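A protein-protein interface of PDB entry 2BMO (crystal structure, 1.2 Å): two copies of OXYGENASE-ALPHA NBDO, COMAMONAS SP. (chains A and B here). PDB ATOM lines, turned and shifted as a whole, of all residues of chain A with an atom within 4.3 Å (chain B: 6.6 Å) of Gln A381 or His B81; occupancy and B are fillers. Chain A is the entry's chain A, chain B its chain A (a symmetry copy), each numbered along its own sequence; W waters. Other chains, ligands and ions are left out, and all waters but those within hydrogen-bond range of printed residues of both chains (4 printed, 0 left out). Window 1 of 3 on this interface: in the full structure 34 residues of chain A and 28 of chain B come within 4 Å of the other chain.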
ATOM      1  N   LEU A  12     -17.409 -27.501  27.133  1.00  0.00           N
ATOM      2  CA  LEU A  12     -17.996 -26.234  27.573  1.00  0.00           C
ATOM      3  C   LEU A  12     -19.324 -25.901  26.891  1.00  0.00           C
ATOM      4  O   LEU A  12     -20.205 -25.292  27.506  1.00  0.00           O
ATOM      5  CB  LEU A  12     -16.995 -25.085  27.373  1.00  0.00           C
ATOM      6  CG  LEU A  12     -17.345 -23.710  27.951  1.00  0.00           C
ATOM      7  CD1 LEU A  12     -17.408 -23.734  29.487  1.00  0.00           C
ATOM      8  CD2 LEU A  12     -16.339 -22.670  27.469  1.00  0.00           C
ATOM      9  N   THR A  13     -19.453 -26.281  25.623  1.00  0.00           N
ATOM     10  CA  THR A  13     -20.686 -26.038  24.882  1.00  0.00           C
ATOM     11  C   THR A  13     -21.085 -27.235  24.043  1.00  0.00           C
ATOM     12  O   THR A  13     -20.242 -28.046  23.656  1.00  0.00           O
ATOM     13  CB  THR A  13     -20.599 -24.773  23.992  1.00  0.00           C
ATOM     14  OG1 THR A  13     -19.638 -24.969  22.949  1.00  0.00           O
ATOM     15  N   GLN A  14     -22.386 -27.344  23.786  1.00  0.00           N
ATOM     16  CA  GLN A  14     -22.939 -28.417  22.972  1.00  0.00           C
ATOM     17  C   GLN A  14     -23.929 -27.814  21.999  1.00  0.00           C
ATOM     18  O   GLN A  14     -24.730 -26.959  22.379  1.00  0.00           O
ATOM     19  CB  GLN A  14     -23.679 -29.445  23.841  1.00  0.00           C
ATOM     20  CG  GLN A  14     -22.854 -30.112  24.937  1.00  0.00           C
ATOM     21  CD  GLN A  14     -22.656 -29.241  26.158  1.00  0.00           C
ATOM     22  OE1 GLN A  14     -23.605 -28.670  26.702  1.00  0.00           O
ATOM     23  NE2 GLN A  14     -21.408 -29.141  26.605  1.00  0.00           N
ATOM     24  N   LEU A  16     -27.298 -27.587  20.290  1.00  0.00           N
ATOM     25  CA  LEU A  16     -28.639 -28.059  20.655  1.00  0.00           C
ATOM     26  C   LEU A  16     -29.145 -29.181  19.732  1.00  0.00           C
ATOM     27  O   LEU A  16     -29.914 -30.051  20.168  1.00  0.00           O
ATOM     28  CB  LEU A  16     -29.614 -26.871  20.700  1.00  0.00           C
ATOM     29  CG  LEU A  16     -30.982 -27.030  21.368  1.00  0.00           C
ATOM     30  CD1 LEU A  16     -30.911 -27.629  22.787  1.00  0.00           C
ATOM     31  CD2 LEU A  16     -31.713 -25.693  21.381  1.00  0.00           C
ATOM     32  N   HIS A  19     -29.711 -33.055  20.489  1.00  0.00           N
ATOM     33  CA  HIS A  19     -30.896 -33.596  21.151  1.00  0.00           C
ATOM     34  C   HIS A  19     -32.068 -33.838  20.209  1.00  0.00           C
ATOM     35  O   HIS A  19     -33.145 -34.249  20.651  1.00  0.00           O
ATOM     36  CB  HIS A  19     -31.303 -32.707  22.323  1.00  0.00           C
ATOM     37  CG  HIS A  19     -30.205 -32.509  23.315  1.00  0.00           C
ATOM     38  ND1 HIS A  19     -29.741 -33.529  24.118  1.00  0.00           N
ATOM     39  CD2 HIS A  19     -29.455 -31.423  23.609  1.00  0.00           C
ATOM     40  CE1 HIS A  19     -28.762 -33.071  24.878  1.00  0.00           C
ATOM     41  NE2 HIS A  19     -28.565 -31.798  24.585  1.00  0.00           N
ATOM     42  N   GLU A 198     -28.054 -35.628  31.121  1.00  0.00           N
ATOM     43  CA  GLU A 198     -27.385 -34.394  31.580  1.00  0.00           C
ATOM     44  C   GLU A 198     -28.050 -33.827  32.831  1.00  0.00           C
ATOM     45  O   GLU A 198     -27.371 -33.354  33.741  1.00  0.00           O
ATOM     46  CB  GLU A 198     -27.279 -33.330  30.473  1.00  0.00           C
ATOM     47  CG  GLU A 198     -28.554 -32.541  30.190  1.00  0.00           C
ATOM     48  CD  GLU A 198     -28.330 -31.334  29.289  1.00  0.00           C
ATOM     49  OE1 GLU A 198     -27.742 -31.511  28.205  1.00  0.00           O
ATOM     50  OE2 GLU A 198     -28.762 -30.211  29.661  1.00  0.00           O
ATOM     51  N   TYR A 205     -28.587 -27.134  39.947  1.00  0.00           N
ATOM     52  CA  TYR A 205     -29.070 -25.778  39.686  1.00  0.00           C
ATOM     53  C   TYR A 205     -30.585 -25.698  39.469  1.00  0.00           C
ATOM     54  O   TYR A 205     -31.215 -24.717  39.867  1.00  0.00           O
ATOM     55  CB  TYR A 205     -28.332 -25.251  38.457  1.00  0.00           C
ATOM     56  CG  TYR A 205     -28.366 -23.757  38.150  1.00  0.00           C
ATOM     57  CD1 TYR A 205     -28.704 -22.790  39.104  1.00  0.00           C
ATOM     58  CD2 TYR A 205     -27.987 -23.321  36.888  1.00  0.00           C
ATOM     59  CE1 TYR A 205     -28.694 -21.419  38.770  1.00  0.00           C
ATOM     60  CE2 TYR A 205     -27.958 -21.978  36.553  1.00  0.00           C
ATOM     61  CZ  TYR A 205     -28.310 -21.038  37.485  1.00  0.00           C
ATOM     62  OH  TYR A 205     -28.262 -19.713  37.109  1.00  0.00           O
ATOM     63  N   MET A 367     -36.431 -28.870  25.237  1.00  0.00           N
ATOM     64  CA  MET A 367     -35.033 -28.860  24.852  1.00  0.00           C
ATOM     65  C   MET A 367     -34.860 -29.750  23.639  1.00  0.00           C
ATOM     66  O   MET A 367     -34.307 -29.334  22.618  1.00  0.00           O
ATOM     67  CB  MET A 367     -34.146 -29.370  25.984  1.00  0.00           C
ATOM     68  CG  MET A 367     -32.724 -29.757  25.543  1.00  0.00           C
ATOM     69  SD  MET A 367     -31.757 -30.405  26.907  1.00  0.00           S
ATOM     70  CE  MET A 367     -32.165 -29.146  28.101  1.00  0.00           C
ATOM     71  N   ILE A 379     -28.259 -23.115  18.038  1.00  0.00           N
ATOM     72  CA  ILE A 379     -27.958 -22.472  19.322  1.00  0.00           C
ATOM     73  C   ILE A 379     -27.122 -23.426  20.178  1.00  0.00           C
ATOM     74  O   ILE A 379     -27.384 -24.630  20.195  1.00  0.00           O
ATOM     75  CB  ILE A 379     -29.252 -22.045  20.057  1.00  0.00           C
ATOM     76  CG1 ILE A 379     -29.964 -20.962  19.245  1.00  0.00           C
ATOM     77  CG2 ILE A 379     -28.954 -21.544  21.486  1.00  0.00           C
ATOM     78  CD1 ILE A 379     -31.377 -20.683  19.686  1.00  0.00           C
ATOM     79  N   ASP A 380     -26.107 -22.891  20.857  1.00  0.00           N
ATOM     80  CA  ASP A 380     -25.312 -23.682  21.799  1.00  0.00           C
ATOM     81  C   ASP A 380     -25.978 -23.775  23.162  1.00  0.00           C
ATOM     82  O   ASP A 380     -26.505 -22.785  23.681  1.00  0.00           O
ATOM     83  CB  ASP A 380     -23.937 -23.048  22.029  1.00  0.00           C
ATOM     84  CG  ASP A 380     -23.004 -23.184  20.849  1.00  0.00           C
ATOM     85  OD1 ASP A 380     -23.184 -24.094  20.015  1.00  0.00           O
ATOM     86  OD2 ASP A 380     -22.053 -22.370  20.778  1.00  0.00           O
ATOM     87  N   GLN A 381     -25.954 -24.971  23.744  1.00  0.00           N
ATOM     88  CA  GLN A 381     -26.095 -25.115  25.187  1.00  0.00           C
ATOM     89  C   GLN A 381     -24.753 -24.784  25.815  1.00  0.00           C
ATOM     90  O   GLN A 381     -23.706 -25.151  25.268  1.00  0.00           O
ATOM     91  CB  GLN A 381     -26.443 -26.549  25.565  1.00  0.00           C
ATOM     92  CG  GLN A 381     -27.675 -27.118  24.886  1.00  0.00           C
ATOM     93  CD  GLN A 381     -27.915 -28.550  25.308  1.00  0.00           C
ATOM     94  OE1 GLN A 381     -27.137 -29.447  24.962  1.00  0.00           O
ATOM     95  NE2 GLN A 381     -28.974 -28.770  26.089  1.00  0.00           N
ATOM     96  N   ILE A 382     -24.781 -24.122  26.964  1.00  0.00           N
ATOM     97  CA  ILE A 382     -23.539 -23.797  27.658  1.00  0.00           C
ATOM     98  C   ILE A 382     -23.455 -24.512  28.998  1.00  0.00           C
ATOM     99  O   ILE A 382     -24.441 -24.598  29.738  1.00  0.00           O
ATOM    100  CB  ILE A 382     -23.327 -22.270  27.802  1.00  0.00           C
ATOM    101  CG1 ILE A 382     -24.385 -21.632  28.700  1.00  0.00           C
ATOM    102  CG2 ILE A 382     -23.298 -21.611  26.432  1.00  0.00           C
ATOM    103  CD1 ILE A 382     -23.908 -20.354  29.370  1.00  0.00           C
ATOM    104  N   ALA A 383     -22.270 -25.039  29.289  1.00  0.00           N
ATOM    105  CA  ALA A 383     -22.037 -25.792  30.520  1.00  0.00           C
ATOM    106  C   ALA A 383     -20.869 -25.142  31.251  1.00  0.00           C
ATOM    107  O   ALA A 383     -19.840 -25.775  31.501  1.00  0.00           O
ATOM    108  CB  ALA A 383     -21.760 -27.270  30.212  1.00  0.00           C
ATOM    109  N   GLU A 408     -21.550 -27.344  36.776  1.00  0.00           N
ATOM    110  CA  GLU A 408     -21.617 -28.064  35.510  1.00  0.00           C
ATOM    111  C   GLU A 408     -20.331 -28.848  35.194  1.00  0.00           C
ATOM    112  O   GLU A 408     -20.106 -29.283  34.070  1.00  0.00           O
ATOM    113  CB  GLU A 408     -22.085 -27.119  34.389  1.00  0.00           C
ATOM    114  CG  GLU A 408     -23.587 -26.802  34.534  1.00  0.00           C
ATOM    115  CD  GLU A 408     -24.072 -25.536  33.845  1.00  0.00           C
ATOM    116  OE1 GLU A 408     -23.267 -24.736  33.322  1.00  0.00           O
ATOM    117  OE2 GLU A 408     -25.304 -25.327  33.841  1.00  0.00           O
ATOM    118  N   VAL B  78     -36.093 -19.710  22.708  1.00  0.00           N
ATOM    119  CA  VAL B  78     -35.132 -20.707  23.166  1.00  0.00           C
ATOM    120  C   VAL B  78     -34.171 -20.058  24.152  1.00  0.00           C
ATOM    121  O   VAL B  78     -33.498 -19.075  23.836  1.00  0.00           O
ATOM    122  CB  VAL B  78     -34.312 -21.305  21.979  1.00  0.00           C
ATOM    123  CG1 VAL B  78     -33.326 -22.367  22.479  1.00  0.00           C
ATOM    124  CG2 VAL B  78     -35.228 -21.898  20.906  1.00  0.00           C
ATOM    125  N   CYS B  79     -34.096 -20.629  25.348  1.00  0.00           N
ATOM    126  CA  CYS B  79     -33.158 -20.148  26.354  1.00  0.00           C
ATOM    127  C   CYS B  79     -31.699 -20.413  25.945  1.00  0.00           C
ATOM    128  O   CYS B  79     -31.381 -21.466  25.392  1.00  0.00           O
ATOM    129  CB  CYS B  79     -33.471 -20.813  27.696  1.00  0.00           C
ATOM    130  SG  CYS B  79     -32.447 -20.216  29.069  1.00  0.00           S
ATOM    131  N   ARG B  80     -30.824 -19.446  26.218  1.00  0.00           N
ATOM    132  CA  ARG B  80     -29.401 -19.548  25.873  1.00  0.00           C
ATOM    133  C   ARG B  80     -28.574 -20.393  26.844  1.00  0.00           C
ATOM    134  O   ARG B  80     -27.366 -20.557  26.649  1.00  0.00           O
ATOM    135  CB  ARG B  80     -28.783 -18.151  25.769  1.00  0.00           C
ATOM    136  CG  ARG B  80     -29.308 -17.312  24.611  1.00  0.00           C
ATOM    137  CD  ARG B  80     -28.816 -17.791  23.237  1.00  0.00           C
ATOM    138  NE  ARG B  80     -27.366 -17.988  23.169  1.00  0.00           N
ATOM    139  CZ  ARG B  80     -26.462 -17.029  22.963  1.00  0.00           C
ATOM    140  NH1 ARG B  80     -26.829 -15.761  22.818  1.00  0.00           N
ATOM    141  NH2 ARG B  80     -25.172 -17.335  22.910  1.00  0.00           N
ATOM    142  N   HIS B  81     -29.204 -20.913  27.890  1.00  0.00           N
ATOM    143  CA  HIS B  81     -28.490 -21.757  28.844  1.00  0.00           C
ATOM    144  C   HIS B  81     -28.461 -23.216  28.371  1.00  0.00           C
ATOM    145  O   HIS B  81     -27.420 -23.691  27.904  1.00  0.00           O
ATOM    146  CB  HIS B  81     -29.075 -21.589  30.245  1.00  0.00           C
ATOM    147  CG  HIS B  81     -28.441 -22.457  31.284  1.00  0.00           C
ATOM    148  ND1 HIS B  81     -29.179 -23.068  32.274  1.00  0.00           N
ATOM    149  CD2 HIS B  81     -27.150 -22.818  31.490  1.00  0.00           C
ATOM    150  CE1 HIS B  81     -28.365 -23.765  33.052  1.00  0.00           C
ATOM    151  NE2 HIS B  81     -27.132 -23.630  32.597  1.00  0.00           N
ATOM    152  N   ARG B  82     -29.582 -23.929  28.487  1.00  0.00           N
ATOM    153  CA  ARG B  82     -29.648 -25.327  28.042  1.00  0.00           C
ATOM    154  C   ARG B  82     -30.664 -25.543  26.916  1.00  0.00           C
ATOM    155  O   ARG B  82     -30.920 -26.669  26.515  1.00  0.00           O
ATOM    156  CB  ARG B  82     -29.950 -26.289  29.214  1.00  0.00           C
ATOM    157  CG  ARG B  82     -28.985 -26.246  30.415  1.00  0.00           C
ATOM    158  CD  ARG B  82     -27.529 -26.509  30.052  1.00  0.00           C
ATOM    159  NE  ARG B  82     -27.307 -27.780  29.361  1.00  0.00           N
ATOM    160  CZ  ARG B  82     -26.175 -28.085  28.723  1.00  0.00           C
ATOM    161  NH1 ARG B  82     -25.170 -27.219  28.695  1.00  0.00           N
ATOM    162  NH2 ARG B  82     -26.042 -29.254  28.102  1.00  0.00           N
ATOM    163  N   GLY B  83     -31.260 -24.468  26.410  1.00  0.00           N
ATOM    164  CA  GLY B  83     -32.088 -24.570  25.215  1.00  0.00           C
ATOM    165  C   GLY B  83     -33.553 -24.912  25.405  1.00  0.00           C
ATOM    166  O   GLY B  83     -34.230 -25.305  24.448  1.00  0.00           O
ATOM    167  N   LYS B  84     -34.040 -24.770  26.632  1.00  0.00           N
ATOM    168  CA  LYS B  84     -35.464 -24.929  26.913  1.00  0.00           C
ATOM    169  C   LYS B  84     -36.299 -23.855  26.197  1.00  0.00           C
ATOM    170  O   LYS B  84     -35.866 -22.713  26.041  1.00  0.00           O
ATOM    171  CB  LYS B  84     -35.724 -24.849  28.420  1.00  0.00           C
ATOM    172  CG  LYS B  84     -37.073 -25.431  28.848  1.00  0.00           C
ATOM    173  CD  LYS B  84     -37.569 -24.817  30.139  1.00  0.00           C
ATOM    174  CE  LYS B  84     -39.026 -25.157  30.374  1.00  0.00           C
ATOM    175  NZ  LYS B  84     -39.929 -24.186  29.693  1.00  0.00           N
ATOM    176  N   CYS B  99     -37.021 -18.148  32.292  1.00  0.00           N
ATOM    177  CA  CYS B  99     -36.936 -19.554  31.945  1.00  0.00           C
ATOM    178  C   CYS B  99     -37.272 -20.426  33.149  1.00  0.00           C
ATOM    179  O   CYS B  99     -36.690 -20.270  34.222  1.00  0.00           O
ATOM    180  CB  CYS B  99     -35.543 -19.882  31.430  1.00  0.00           C
ATOM    181  SG  CYS B  99     -35.426 -21.605  30.899  1.00  0.00           S
ATOM    182  N   TYR B 101     -36.577 -23.479  33.762  1.00  0.00           N
ATOM    183  CA  TYR B 101     -35.653 -24.558  34.101  1.00  0.00           C
ATOM    184  C   TYR B 101     -34.769 -24.127  35.284  1.00  0.00           C
ATOM    185  O   TYR B 101     -34.876 -24.698  36.380  1.00  0.00           O
ATOM    186  CB  TYR B 101     -34.859 -24.946  32.853  1.00  0.00           C
ATOM    187  CG  TYR B 101     -34.154 -26.299  32.870  1.00  0.00           C
ATOM    188  CD1 TYR B 101     -33.604 -26.803  31.694  1.00  0.00           C
ATOM    189  CD2 TYR B 101     -34.027 -27.064  34.038  1.00  0.00           C
ATOM    190  CE1 TYR B 101     -32.930 -28.035  31.673  1.00  0.00           C
ATOM    191  CE2 TYR B 101     -33.357 -28.299  34.023  1.00  0.00           C
ATOM    192  CZ  TYR B 101     -32.815 -28.772  32.842  1.00  0.00           C
ATOM    193  OH  TYR B 101     -32.147 -29.980  32.812  1.00  0.00           O
ATOM    194  N   HIS B 102     -33.924 -23.111  35.076  1.00  0.00           N
ATOM    195  CA  HIS B 102     -33.015 -22.634  36.134  1.00  0.00           C
ATOM    196  C   HIS B 102     -33.273 -21.204  36.587  1.00  0.00           C
ATOM    197  O   HIS B 102     -32.679 -20.753  37.565  1.00  0.00           O
ATOM    198  CB  HIS B 102     -31.544 -22.802  35.746  1.00  0.00           C
ATOM    199  CG  HIS B 102     -31.229 -24.153  35.199  1.00  0.00           C
ATOM    200  ND1 HIS B 102     -31.315 -24.445  33.855  1.00  0.00           N
ATOM    201  CD2 HIS B 102     -30.862 -25.303  35.820  1.00  0.00           C
ATOM    202  CE1 HIS B 102     -30.995 -25.717  33.671  1.00  0.00           C
ATOM    203  NE2 HIS B 102     -30.726 -26.262  34.847  1.00  0.00           N
ATOM    204  N   TRP B 104     -33.173 -18.208  34.574  1.00  0.00           N
ATOM    205  CA  TRP B 104     -32.595 -17.069  33.843  1.00  0.00           C
ATOM    206  C   TRP B 104     -33.719 -16.147  33.382  1.00  0.00           C
ATOM    207  O   TRP B 104     -34.740 -16.615  32.856  1.00  0.00           O
ATOM    208  CB  TRP B 104     -31.793 -17.535  32.638  1.00  0.00           C
ATOM    209  CG  TRP B 104     -30.443 -18.117  32.964  1.00  0.00           C
ATOM    210  CD1 TRP B 104     -30.032 -18.656  34.158  1.00  0.00           C
ATOM    211  CD2 TRP B 104     -29.345 -18.263  32.064  1.00  0.00           C
ATOM    212  NE1 TRP B 104     -28.736 -19.106  34.051  1.00  0.00           N
ATOM    213  CE2 TRP B 104     -28.291 -18.874  32.778  1.00  0.00           C
ATOM    214  CE3 TRP B 104     -29.140 -17.911  30.722  1.00  0.00           C
ATOM    215  CZ2 TRP B 104     -27.058 -19.157  32.194  1.00  0.00           C
ATOM    216  CZ3 TRP B 104     -27.910 -18.195  30.137  1.00  0.00           C
ATOM    217  CH2 TRP B 104     -26.886 -18.815  30.876  1.00  0.00           C
ATOM    218  N   TYR B 106     -34.871 -12.849  31.073  1.00  0.00           N
ATOM    219  CA  TYR B 106     -34.572 -12.002  29.929  1.00  0.00           C
ATOM    220  C   TYR B 106     -35.532 -10.833  29.884  1.00  0.00           C
ATOM    221  O   TYR B 106     -36.673 -10.941  30.321  1.00  0.00           O
ATOM    222  CB  TYR B 106     -34.725 -12.790  28.627  1.00  0.00           C
ATOM    223  CG  TYR B 106     -33.823 -14.000  28.528  1.00  0.00           C
ATOM    224  CD1 TYR B 106     -34.218 -15.230  29.059  1.00  0.00           C
ATOM    225  CD2 TYR B 106     -32.577 -13.922  27.912  1.00  0.00           C
ATOM    226  CE1 TYR B 106     -33.413 -16.344  28.971  1.00  0.00           C
ATOM    227  CE2 TYR B 106     -31.751 -15.054  27.821  1.00  0.00           C
ATOM    228  CZ  TYR B 106     -32.200 -16.258  28.353  1.00  0.00           C
ATOM    229  OH  TYR B 106     -31.419 -17.382  28.261  1.00  0.00           O
ATOM    230  N   TYR B 122     -21.316 -17.952  39.567  1.00  0.00           N
ATOM    231  CA  TYR B 122     -20.784 -17.608  38.252  1.00  0.00           C
ATOM    232  C   TYR B 122     -19.605 -16.642  38.316  1.00  0.00           C
ATOM    233  O   TYR B 122     -18.549 -16.927  37.759  1.00  0.00           O
ATOM    234  CB  TYR B 122     -21.870 -17.039  37.336  1.00  0.00           C
ATOM    235  CG  TYR B 122     -22.706 -18.069  36.605  1.00  0.00           C
ATOM    236  CD1 TYR B 122     -24.013 -18.327  37.002  1.00  0.00           C
ATOM    237  CD2 TYR B 122     -22.200 -18.764  35.503  1.00  0.00           C
ATOM    238  CE1 TYR B 122     -24.799 -19.252  36.333  1.00  0.00           C
ATOM    239  CE2 TYR B 122     -22.983 -19.708  34.824  1.00  0.00           C
ATOM    240  CZ  TYR B 122     -24.286 -19.938  35.252  1.00  0.00           C
ATOM    241  OH  TYR B 122     -25.097 -20.851  34.608  1.00  0.00           O
ATOM    242  N   LEU B 131     -25.163 -13.540  25.925  1.00  0.00           N
ATOM    243  CA  LEU B 131     -26.158 -14.593  26.127  1.00  0.00           C
ATOM    244  C   LEU B 131     -27.595 -14.086  25.973  1.00  0.00           C
ATOM    245  O   LEU B 131     -28.535 -14.661  26.542  1.00  0.00           O
ATOM    246  CB  LEU B 131     -25.945 -15.254  27.490  1.00  0.00           C
ATOM    247  CG  LEU B 131     -24.693 -16.124  27.628  1.00  0.00           C
ATOM    248  CD1 LEU B 131     -24.407 -16.372  29.093  1.00  0.00           C
ATOM    249  CD2 LEU B 131     -24.881 -17.433  26.873  1.00  0.00           C
HETATM  250  O   HOH W   1     -29.130 -23.274  24.863  1.00  0.00           O
HETATM  251  O   HOH W   2     -29.546 -29.293  32.213  1.00  0.00           O
HETATM  252  O   HOH W   3     -23.968 -22.224  32.554  1.00  0.00           O
HETATM  253  O   HOH W   4     -26.051 -20.226  24.339  1.00  0.00           O
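The guanidinium group of Arg B82 lies within hydrogen-bond range of the side-chain amide oxygen of Gln A14 (2.9 Å).
NH2 of Arg B82 is in salt-bridge range of OE1 of Glu A198, 2.8 Å away.
The side-chain hydroxyl (OH) of Tyr A205 is in hydrogen-bond range of the indole nitrogen (NE1) of Trp B104, at 3.2 Å.
The backbone carbonyl oxygen (O) of Arg B82 is in hydrogen-bond range of the side-chain amide nitrogen (NE2) of Gln A381 (2.9 Å).
The backbone carbonyl oxygen (O) of His B81 sits at hydrogen-bond distance from the backbone NH (N) of Ile A382.
The guanidinium group (NH1) of Arg B82 lies within hydrogen-bond range of the backbone carbonyl oxygen (O) of Ile A382 (2.9 Å).
A ring nitrogen (NE2) of His B81 is in hydrogen-bond range of the side-chain carboxylate of Glu A408 (2.8 Å).
Gln A381 touches just these residues of chain B: His B81 (3.3 Å) and Arg B82 (2.9 Å).
Of the printed residues of chain B, Gln A14 touches Arg B82 (2.9 Å).
Printed residues of chain A within 4 Å of Val B78: Leu A16 and Ile A379.
Lys B84 touches none of the printed residues of chain A.
Cys B99 touches none of the printed residues of chain A.
The nearest residue of chain B that does not touch Gln A381 is Gly B83 (4.7 Å).
The nearest printed residue of chain A that does not touch His B81 is Asp A380 (4.4 Å).
N of Leu A16 lies within hydrogen-bond range of O of Ile A379, at 3.0 Å.
NE2 of His A19 lies within hydrogen-bond range of OE1 of Gln A381, at 2.8 Å.
The side-chain amide nitrogen (NE2) of Gln A381 sits at hydrogen-bond distance from the side-chain sulfur (SD) of Met A367 (3.3 Å).
The side-chain sulfur (SG) of Cys B79 sits close to the backbone NH (N) of His B81 (3.5 Å).
The side-chain sulfur of Cys B99 sits close to the backbone NH of Tyr B101, 3.6 Å away.
N of Cys B99 is in hydrogen-bond range of O of Trp B104 (2.8 Å).
Water W4 lies within hydrogen-bond range of O of Arg B80 (2.7 Å) and O of Asp A380 (2.7 Å).
Water W3 lies within hydrogen-bond range of OH of Tyr B122 (2.7 Å), OE1 of Glu A408 (2.7 Å) and NE2 of His B81 (3.5 Å).
Water W2 bridges OH of Tyr B101 and OE2 of Glu A198.
Water W1 lies within hydrogen-bond range of N of Gly B83 (2.9 Å), O of Asp A380 (2.9 Å) and O of Cys B79 (2.9 Å).
No position is printed for both chains.
Of the 23 pairs that touch across the chains among the printed residues, none has its exchanged pair printed and touching as well.
Of the 14 printed residues of chain A, 11 touch a printed residue of chain B.
Printed residues of chain A that touch a printed residue of chain B: Gln A14, Leu A16, Glu A198, Tyr A205, Met A367, Ile A379, Asp A380, Gln A381, Ile A382, Ala A383 and Glu A408.
Hydrophobic or aromatic side chains of chain A that line the printed part of chain B: Leu A16, Tyr A205, Met A367, Ile A379, Ile A382 and Ala A383.
Of the 14 printed residues of chain B, 10 touch a printed residue of chain A.
Hydrophobic or aromatic side chains of chain B within 4 Å of the printed part of chain A: Val B78, His B81, Tyr B101, His B102, Trp B104, Tyr B122 and Leu B131.
Among the printed residues, merely in contact across the chains: Leu A16 with Val B78, Leu A16 with Arg B82, Leu A16 with Gly B83, Tyr A205 with His B81, Tyr A205 with His B102, Tyr A205 with Tyr B122, Met A367 with Arg B82, Met A367 with Gly B83, Met A367 with Tyr B101, Ile A379 with Val B78, Asp A380 with Arg B80, Gln A381 with His B81, Ile A382 with Arg B80, Ile A382 with Trp B104, Ile A382 with Leu B131 and Ala A383 with Arg B82.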
